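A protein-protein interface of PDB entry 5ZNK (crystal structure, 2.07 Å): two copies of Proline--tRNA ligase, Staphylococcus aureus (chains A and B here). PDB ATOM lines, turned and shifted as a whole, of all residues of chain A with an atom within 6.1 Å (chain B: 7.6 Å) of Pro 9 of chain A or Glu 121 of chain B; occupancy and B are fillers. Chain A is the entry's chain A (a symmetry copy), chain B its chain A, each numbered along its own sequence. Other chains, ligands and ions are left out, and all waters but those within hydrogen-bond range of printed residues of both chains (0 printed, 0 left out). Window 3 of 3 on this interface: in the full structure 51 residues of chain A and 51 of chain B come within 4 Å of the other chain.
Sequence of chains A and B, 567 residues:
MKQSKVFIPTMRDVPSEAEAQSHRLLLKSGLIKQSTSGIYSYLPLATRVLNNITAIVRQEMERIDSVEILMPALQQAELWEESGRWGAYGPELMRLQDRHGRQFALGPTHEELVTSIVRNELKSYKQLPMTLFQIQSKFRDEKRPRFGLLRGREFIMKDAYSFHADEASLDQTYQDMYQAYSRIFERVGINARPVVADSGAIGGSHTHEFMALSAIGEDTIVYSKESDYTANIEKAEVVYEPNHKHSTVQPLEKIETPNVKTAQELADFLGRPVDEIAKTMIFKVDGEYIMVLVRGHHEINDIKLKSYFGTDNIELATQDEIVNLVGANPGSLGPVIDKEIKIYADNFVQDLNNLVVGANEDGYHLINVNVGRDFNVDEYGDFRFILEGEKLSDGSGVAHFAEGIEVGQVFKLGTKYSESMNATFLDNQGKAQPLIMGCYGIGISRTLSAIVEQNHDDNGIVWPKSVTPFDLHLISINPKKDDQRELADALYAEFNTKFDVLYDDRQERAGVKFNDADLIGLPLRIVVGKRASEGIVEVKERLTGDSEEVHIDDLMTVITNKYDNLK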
ATOM      1  N   PHE A   7      -4.891   7.527 -18.794  1.00  0.00           N
ATOM      2  CA  PHE A   7      -5.759   7.638 -19.955  1.00  0.00           C
ATOM      3  C   PHE A   7      -7.198   7.245 -19.586  1.00  0.00           C
ATOM      4  O   PHE A   7      -7.475   6.078 -19.290  1.00  0.00           O
ATOM      5  CB  PHE A   7      -5.226   6.743 -21.076  1.00  0.00           C
ATOM      6  CG  PHE A   7      -5.951   6.899 -22.379  1.00  0.00           C
ATOM      7  CD1 PHE A   7      -5.967   8.128 -23.036  1.00  0.00           C
ATOM      8  CD2 PHE A   7      -6.605   5.821 -22.963  1.00  0.00           C
ATOM      9  CE1 PHE A   7      -6.635   8.277 -24.238  1.00  0.00           C
ATOM     10  CE2 PHE A   7      -7.262   5.961 -24.167  1.00  0.00           C
ATOM     11  CZ  PHE A   7      -7.284   7.191 -24.806  1.00  0.00           C
ATOM     12  N   ILE A   8      -8.088   8.242 -19.564  1.00  0.00           N
ATOM     13  CA  ILE A   8      -9.504   8.069 -19.218  1.00  0.00           C
ATOM     14  C   ILE A   8     -10.323   8.944 -20.180  1.00  0.00           C
ATOM     15  O   ILE A   8     -10.710  10.062 -19.822  1.00  0.00           O
ATOM     16  CB  ILE A   8      -9.822   8.476 -17.751  1.00  0.00           C
ATOM     17  CG1 ILE A   8      -8.827   7.848 -16.769  1.00  0.00           C
ATOM     18  CG2 ILE A   8     -11.258   8.078 -17.405  1.00  0.00           C
ATOM     19  CD1 ILE A   8      -9.000   8.259 -15.315  1.00  0.00           C
ATOM     20  N   PRO A   9     -10.582   8.447 -21.408  1.00  0.00           N
ATOM     21  CA  PRO A   9     -11.244   9.250 -22.445  1.00  0.00           C
ATOM     22  C   PRO A   9     -12.762   9.304 -22.240  1.00  0.00           C
ATOM     23  O   PRO A   9     -13.536   8.638 -22.938  1.00  0.00           O
ATOM     24  CB  PRO A   9     -10.863   8.519 -23.730  1.00  0.00           C
ATOM     25  CG  PRO A   9     -10.784   7.089 -23.311  1.00  0.00           C
ATOM     26  CD  PRO A   9     -10.263   7.091 -21.900  1.00  0.00           C
ATOM     27  N   THR A  10     -13.162  10.083 -21.247  1.00  0.00           N
ATOM     28  CA  THR A  10     -14.561  10.292 -20.914  1.00  0.00           C
ATOM     29  C   THR A  10     -15.298  10.913 -22.104  1.00  0.00           C
ATOM     30  O   THR A  10     -14.748  11.770 -22.783  1.00  0.00           O
ATOM     31  CB  THR A  10     -14.672  11.227 -19.693  1.00  0.00           C
ATOM     32  OG1 THR A  10     -14.085  10.582 -18.558  1.00  0.00           O
ATOM     33  CG2 THR A  10     -16.107  11.527 -19.380  1.00  0.00           C
ATOM     34  N   MET A  11     -16.528  10.466 -22.345  1.00  0.00           N
ATOM     35  CA  MET A  11     -17.359  10.979 -23.443  1.00  0.00           C
ATOM     36  C   MET A  11     -18.428  11.935 -22.929  1.00  0.00           C
ATOM     37  O   MET A  11     -18.889  11.815 -21.793  1.00  0.00           O
ATOM     38  CB  MET A  11     -18.053   9.837 -24.194  1.00  0.00           C
ATOM     39  CG  MET A  11     -17.117   8.774 -24.754  1.00  0.00           C
ATOM     40  SD  MET A  11     -17.976   7.489 -25.703  1.00  0.00           S
ATOM     41  CE  MET A  11     -16.578   6.559 -26.335  1.00  0.00           C
ATOM     42  N   LEU A  27     -18.280   2.729 -22.008  1.00  0.00           N
ATOM     43  CA  LEU A  27     -17.871   3.682 -23.049  1.00  0.00           C
ATOM     44  C   LEU A  27     -17.766   5.113 -22.512  1.00  0.00           C
ATOM     45  O   LEU A  27     -16.731   5.769 -22.666  1.00  0.00           O
ATOM     46  CB  LEU A  27     -18.843   3.650 -24.238  1.00  0.00           C
ATOM     47  CG  LEU A  27     -18.867   2.379 -25.106  1.00  0.00           C
ATOM     48  CD1 LEU A  27     -20.028   2.424 -26.093  1.00  0.00           C
ATOM     49  CD2 LEU A  27     -17.552   2.187 -25.851  1.00  0.00           C
ATOM     50  N   LYS A  28     -18.841   5.592 -21.891  1.00  0.00           N
ATOM     51  CA  LYS A  28     -18.922   6.983 -21.471  1.00  0.00           C
ATOM     52  C   LYS A  28     -17.858   7.351 -20.439  1.00  0.00           C
ATOM     53  O   LYS A  28     -17.314   8.446 -20.487  1.00  0.00           O
ATOM     54  CB  LYS A  28     -20.312   7.287 -20.914  1.00  0.00           C
ATOM     55  CG  LYS A  28     -20.652   8.767 -20.821  1.00  0.00           C
ATOM     56  CD  LYS A  28     -22.100   8.949 -20.367  1.00  0.00           C
ATOM     57  CE  LYS A  28     -22.396  10.368 -19.918  1.00  0.00           C
ATOM     58  NZ  LYS A  28     -22.340  11.322 -21.052  1.00  0.00           N
ATOM     59  N   SER A  29     -17.562   6.424 -19.529  1.00  0.00           N
ATOM     60  CA  SER A  29     -16.555   6.633 -18.481  1.00  0.00           C
ATOM     61  C   SER A  29     -15.092   6.410 -18.913  1.00  0.00           C
ATOM     62  O   SER A  29     -14.184   6.522 -18.091  1.00  0.00           O
ATOM     63  CB  SER A  29     -16.870   5.752 -17.263  1.00  0.00           C
ATOM     64  OG  SER A  29     -16.803   4.370 -17.587  1.00  0.00           O
ATOM     65  N   GLY A  30     -14.860   6.102 -20.185  1.00  0.00           N
ATOM     66  CA  GLY A  30     -13.512   5.893 -20.701  1.00  0.00           C
ATOM     67  C   GLY A  30     -12.848   4.625 -20.207  1.00  0.00           C
ATOM     68  O   GLY A  30     -11.653   4.620 -19.929  1.00  0.00           O
ATOM     69  N   LEU A  31     -13.611   3.544 -20.095  1.00  0.00           N
ATOM     70  CA  LEU A  31     -13.073   2.265 -19.602  1.00  0.00           C
ATOM     71  C   LEU A  31     -12.772   1.224 -20.679  1.00  0.00           C
ATOM     72  O   LEU A  31     -11.860   0.430 -20.509  1.00  0.00           O
ATOM     73  CB  LEU A  31     -13.995   1.662 -18.537  1.00  0.00           C
ATOM     74  CG  LEU A  31     -13.508   1.949 -17.113  1.00  0.00           C
ATOM     75  CD1 LEU A  31     -13.515   3.443 -16.821  1.00  0.00           C
ATOM     76  CD2 LEU A  31     -14.359   1.227 -16.087  1.00  0.00           C
ATOM     77  N   ILE A  32     -13.556   1.205 -21.749  1.00  0.00           N
ATOM     78  CA  ILE A  32     -13.299   0.323 -22.895  1.00  0.00           C
ATOM     79  C   ILE A  32     -13.328   1.123 -24.178  1.00  0.00           C
ATOM     80  O   ILE A  32     -13.877   2.203 -24.227  1.00  0.00           O
ATOM     81  CB  ILE A  32     -14.276  -0.892 -22.973  1.00  0.00           C
ATOM     82  CG1 ILE A  32     -15.717  -0.437 -23.247  1.00  0.00           C
ATOM     83  CG2 ILE A  32     -14.161  -1.719 -21.698  1.00  0.00           C
ATOM     84  CD1 ILE A  32     -16.741  -1.550 -23.376  1.00  0.00           C
ATOM     85  N   LYS A  33     -12.709   0.582 -25.217  1.00  0.00           N
ATOM     86  CA  LYS A  33     -12.830   1.134 -26.561  1.00  0.00           C
ATOM     87  C   LYS A  33     -12.936  -0.015 -27.542  1.00  0.00           C
ATOM     88  O   LYS A  33     -12.120  -0.939 -27.504  1.00  0.00           O
ATOM     89  CB  LYS A  33     -11.640   2.041 -26.908  1.00  0.00           C
ATOM     90  CG  LYS A  33     -11.731   2.670 -28.290  1.00  0.00           C
ATOM     91  CD  LYS A  33     -10.829   3.881 -28.428  1.00  0.00           C
ATOM     92  CE  LYS A  33     -11.079   4.616 -29.737  1.00  0.00           C
ATOM     93  NZ  LYS A  33     -10.295   5.884 -29.857  1.00  0.00           N
ATOM     94  N   LEU A  43      -9.179  -0.204 -21.164  1.00  0.00           N
ATOM     95  CA  LEU A  43      -8.389   0.982 -20.864  1.00  0.00           C
ATOM     96  C   LEU A  43      -8.010   0.947 -19.372  1.00  0.00           C
ATOM     97  O   LEU A  43      -8.404   0.009 -18.663  1.00  0.00           O
ATOM     98  CB  LEU A  43      -9.172   2.211 -21.312  1.00  0.00           C
ATOM     99  CG  LEU A  43      -9.634   2.156 -22.789  1.00  0.00           C
ATOM    100  CD1 LEU A  43     -10.370   3.430 -23.149  1.00  0.00           C
ATOM    101  CD2 LEU A  43      -8.503   1.905 -23.794  1.00  0.00           C
ATOM    102  N   PRO A  44      -7.212   1.915 -18.899  1.00  0.00           N
ATOM    103  CA  PRO A  44      -6.574   1.762 -17.600  1.00  0.00           C
ATOM    104  C   PRO A  44      -7.450   1.364 -16.424  1.00  0.00           C
ATOM    105  O   PRO A  44      -7.094   0.449 -15.697  1.00  0.00           O
ATOM    106  CB  PRO A  44      -5.963   3.145 -17.371  1.00  0.00           C
ATOM    107  CG  PRO A  44      -5.467   3.502 -18.722  1.00  0.00           C
ATOM    108  CD  PRO A  44      -6.576   3.030 -19.645  1.00  0.00           C
ATOM    109  N   THR B 115      -2.145   3.095 -31.249  1.00  0.00           N
ATOM    110  CA  THR B 115      -2.314   4.359 -31.955  1.00  0.00           C
ATOM    111  C   THR B 115      -3.788   4.607 -32.259  1.00  0.00           C
ATOM    112  O   THR B 115      -4.241   5.740 -32.172  1.00  0.00           O
ATOM    113  CB  THR B 115      -1.479   4.385 -33.253  1.00  0.00           C
ATOM    114  OG1 THR B 115      -0.097   4.156 -32.932  1.00  0.00           O
ATOM    115  CG2 THR B 115      -1.597   5.714 -33.971  1.00  0.00           C
ATOM    116  N   SER B 116      -4.510   3.552 -32.630  1.00  0.00           N
ATOM    117  CA  SER B 116      -5.944   3.632 -32.863  1.00  0.00           C
ATOM    118  C   SER B 116      -6.744   3.948 -31.586  1.00  0.00           C
ATOM    119  O   SER B 116      -7.810   4.549 -31.668  1.00  0.00           O
ATOM    120  CB  SER B 116      -6.473   2.357 -33.549  1.00  0.00           C
ATOM    121  OG  SER B 116      -6.581   1.241 -32.668  1.00  0.00           O
ATOM    122  N   ILE B 117      -6.239   3.526 -30.423  1.00  0.00           N
ATOM    123  CA  ILE B 117      -6.861   3.851 -29.138  1.00  0.00           C
ATOM    124  C   ILE B 117      -6.731   5.338 -28.838  1.00  0.00           C
ATOM    125  O   ILE B 117      -7.692   6.019 -28.450  1.00  0.00           O
ATOM    126  CB  ILE B 117      -6.219   3.053 -27.976  1.00  0.00           C
ATOM    127  CG1 ILE B 117      -6.699   1.587 -28.019  1.00  0.00           C
ATOM    128  CG2 ILE B 117      -6.538   3.693 -26.622  1.00  0.00           C
ATOM    129  CD1 ILE B 117      -5.993   0.643 -27.065  1.00  0.00           C
ATOM    130  N   VAL B 118      -5.509   5.811 -29.007  1.00  0.00           N
ATOM    131  CA  VAL B 118      -5.097   7.116 -28.556  1.00  0.00           C
ATOM    132  C   VAL B 118      -5.530   8.245 -29.518  1.00  0.00           C
ATOM    133  O   VAL B 118      -5.664   9.393 -29.092  1.00  0.00           O
ATOM    134  CB  VAL B 118      -3.569   7.058 -28.277  1.00  0.00           C
ATOM    135  CG1 VAL B 118      -2.773   8.165 -28.929  1.00  0.00           C
ATOM    136  CG2 VAL B 118      -3.312   6.928 -26.783  1.00  0.00           C
ATOM    137  N   ARG B 119      -5.752   7.927 -30.793  1.00  0.00           N
ATOM    138  CA  ARG B 119      -5.978   8.975 -31.792  1.00  0.00           C
ATOM    139  C   ARG B 119      -7.344   9.615 -31.594  1.00  0.00           C
ATOM    140  O   ARG B 119      -8.324   8.933 -31.342  1.00  0.00           O
ATOM    141  CB  ARG B 119      -5.810   8.470 -33.224  1.00  0.00           C
ATOM    142  CG  ARG B 119      -6.858   7.495 -33.718  1.00  0.00           C
ATOM    143  CD  ARG B 119      -6.568   7.150 -35.165  1.00  0.00           C
ATOM    144  NE  ARG B 119      -7.248   5.935 -35.587  1.00  0.00           N
ATOM    145  CZ  ARG B 119      -7.037   5.317 -36.743  1.00  0.00           C
ATOM    146  NH1 ARG B 119      -6.155   5.802 -37.621  1.00  0.00           N
ATOM    147  NH2 ARG B 119      -7.702   4.197 -37.021  1.00  0.00           N
ATOM    148  N   ASN B 120      -7.366  10.942 -31.671  1.00  0.00           N
ATOM    149  CA  ASN B 120      -8.553  11.762 -31.360  1.00  0.00           C
ATOM    150  C   ASN B 120      -9.049  11.646 -29.914  1.00  0.00           C
ATOM    151  O   ASN B 120     -10.190  11.989 -29.612  1.00  0.00           O
ATOM    152  CB  ASN B 120      -9.672  11.514 -32.383  1.00  0.00           C
ATOM    153  CG  ASN B 120      -9.317  12.063 -33.752  1.00  0.00           C
ATOM    154  OD1 ASN B 120      -9.303  13.281 -33.959  1.00  0.00           O
ATOM    155  ND2 ASN B 120      -8.998  11.181 -34.684  1.00  0.00           N
ATOM    156  N   GLU B 121      -8.160  11.208 -29.023  1.00  0.00           N
ATOM    157  CA  GLU B 121      -8.438  11.130 -27.593  1.00  0.00           C
ATOM    158  C   GLU B 121      -7.360  11.840 -26.808  1.00  0.00           C
ATOM    159  O   GLU B 121      -7.662  12.570 -25.875  1.00  0.00           O
ATOM    160  CB  GLU B 121      -8.553   9.675 -27.141  1.00  0.00           C
ATOM    161  CG  GLU B 121      -9.673   8.888 -27.807  1.00  0.00           C
ATOM    162  CD  GLU B 121     -11.060   9.488 -27.602  1.00  0.00           C
ATOM    163  OE1 GLU B 121     -11.948   9.180 -28.418  1.00  0.00           O
ATOM    164  OE2 GLU B 121     -11.280  10.264 -26.644  1.00  0.00           O
ATOM    165  N   LEU B 122      -6.102  11.588 -27.159  1.00  0.00           N
ATOM    166  CA  LEU B 122      -5.013  12.499 -26.826  1.00  0.00           C
ATOM    167  C   LEU B 122      -5.074  13.645 -27.842  1.00  0.00           C
ATOM    168  O   LEU B 122      -4.442  13.581 -28.897  1.00  0.00           O
ATOM    169  CB  LEU B 122      -3.655  11.785 -26.858  1.00  0.00           C
ATOM    170  CG  LEU B 122      -3.450  10.636 -25.858  1.00  0.00           C
ATOM    171  CD1 LEU B 122      -2.053  10.038 -25.992  1.00  0.00           C
ATOM    172  CD2 LEU B 122      -3.664  11.076 -24.420  1.00  0.00           C
ATOM    173  N   LYS B 123      -5.865  14.667 -27.504  1.00  0.00           N
ATOM    174  CA  LYS B 123      -6.200  15.791 -28.403  1.00  0.00           C
ATOM    175  C   LYS B 123      -5.327  17.034 -28.221  1.00  0.00           C
ATOM    176  O   LYS B 123      -5.145  17.798 -29.171  1.00  0.00           O
ATOM    177  CB  LYS B 123      -7.661  16.217 -28.193  1.00  0.00           C
ATOM    178  CG  LYS B 123      -8.695  15.115 -28.380  1.00  0.00           C
ATOM    179  N   SER B 124      -4.817  17.230 -27.003  1.00  0.00           N
ATOM    180  CA  SER B 124      -4.096  18.434 -26.598  1.00  0.00           C
ATOM    181  C   SER B 124      -2.737  18.103 -25.976  1.00  0.00           C
ATOM    182  O   SER B 124      -2.561  17.044 -25.363  1.00  0.00           O
ATOM    183  CB  SER B 124      -4.952  19.199 -25.577  1.00  0.00           C
ATOM    184  OG  SER B 124      -4.200  20.128 -24.804  1.00  0.00           O
ATOM    185  N   GLN B 127      -2.542  17.043 -22.209  1.00  0.00           N
ATOM    186  CA  GLN B 127      -2.679  15.639 -21.803  1.00  0.00           C
ATOM    187  C   GLN B 127      -1.394  14.798 -21.937  1.00  0.00           C
ATOM    188  O   GLN B 127      -1.406  13.599 -21.631  1.00  0.00           O
ATOM    189  CB  GLN B 127      -3.777  14.969 -22.631  1.00  0.00           C
ATOM    190  CG  GLN B 127      -5.109  15.696 -22.643  1.00  0.00           C
ATOM    191  CD  GLN B 127      -6.044  15.108 -23.675  1.00  0.00           C
ATOM    192  OE1 GLN B 127      -6.132  15.605 -24.796  1.00  0.00           O
ATOM    193  NE2 GLN B 127      -6.709  14.016 -23.321  1.00  0.00           N
ATOM    194  N   THR B 424      -3.041  13.146 -34.203  1.00  0.00           N
ATOM    195  CA  THR B 424      -2.503  14.470 -33.926  1.00  0.00           C
ATOM    196  C   THR B 424      -3.100  15.083 -32.667  1.00  0.00           C
ATOM    197  O   THR B 424      -4.172  14.699 -32.198  1.00  0.00           O
ATOM    198  CB  THR B 424      -2.731  15.458 -35.096  1.00  0.00           C
ATOM    199  OG1 THR B 424      -4.132  15.691 -35.260  1.00  0.00           O
ATOM    200  CG2 THR B 424      -2.137  14.934 -36.414  1.00  0.00           C
ATOM    201  N   LEU B 435       1.649  12.925 -32.987  1.00  0.00           N
ATOM    202  CA  LEU B 435       2.172  12.410 -31.720  1.00  0.00           C
ATOM    203  C   LEU B 435       3.566  11.794 -31.895  1.00  0.00           C
ATOM    204  O   LEU B 435       3.807  10.999 -32.820  1.00  0.00           O
ATOM    205  CB  LEU B 435       1.228  11.361 -31.106  1.00  0.00           C
ATOM    206  CG  LEU B 435      -0.122  11.874 -30.588  1.00  0.00           C
ATOM    207  CD1 LEU B 435      -1.084  10.718 -30.381  1.00  0.00           C
ATOM    208  CD2 LEU B 435       0.030  12.687 -29.309  1.00  0.00           C
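CE2 of Phe 7 of chain A touches CG2 of Ile 117 of chain B, 3.4 Å away. CZ of Phe 7 of chain A touches CB of Glu 121 of chain B (3.6 Å). Phe 7 of chain A touches Leu 122 of chain B (CD1 to CD2, 3.99 Å). OE2 of Glu 121 of chain B touches CB of Pro 9 of chain A, 3.4 Å away. O of Arg 119 of chain B touches NZ of Lys 33 of chain A (3.9 Å). Leu 43 of chain A touches Ile 117 of chain B (CD2 to CG2, 3.9 Å).
No position is printed for both chains. Of the 9 pairs that touch across the chains among the printed residues, none has its exchanged pair printed and touching as well.
Pro 9 of chain A touches one residue of chain B. Glu 121 of chain B touches just these residues of chain A: Phe 7, Pro 9 and Lys 33. Printed residues of chain B within 4 Å of Leu 43 of chain A: Ile 117. Of the printed residues of chain B, Phe 7 of chain A touches Ile 117, Glu 121 and Leu 122. Of the printed residues of chain A, Ile 117 of chain B touches Phe 7, Lys 33 and Leu 43. Of the printed residues of chain B, Lys 33 of chain A touches Ser 116, Ile 117, Arg 119 and Glu 121. Thr 115 of chain B touches none of the printed residues of chain A. The nearest residue of chain B that does not touch Pro 9 of chain A is Ile 117 of chain B (6.1 Å).
Hydrophobic or aromatic side chains of chain B that line the printed part of chain A: Ile 117 and Leu 122. Among the printed residues, 9 pairs touch across the chains. Among the printed residues, Asp or Glu carboxylates within 4 Å of a Lys or Arg side-chain nitrogen of the other chain: Lys 33 of chain A with Glu 121 of chain B (3.96 Å).
O of Glu 121 of chain B is in hydrogen-bond range of NE2 of Gln 127 of chain B (3.1 Å). O of Leu 31 of chain A sits at hydrogen-bond distance from N of Leu 43 of chain A (2.8 Å).
The side-chain amino group (NZ) of Lys 33 of chain A lies within hydrogen-bond range of the backbone carbonyl oxygen (O) of Ser 116 of chain B (3.4 Å). O of Ile 117 of chain B sits at hydrogen-bond distance from NZ of Lys 33 of chain A, 3.0 Å away. OE1 of Glu 121 of chain B is in salt-bridge range of NZ of Lys 33 of chain A, 3.96 Å away.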
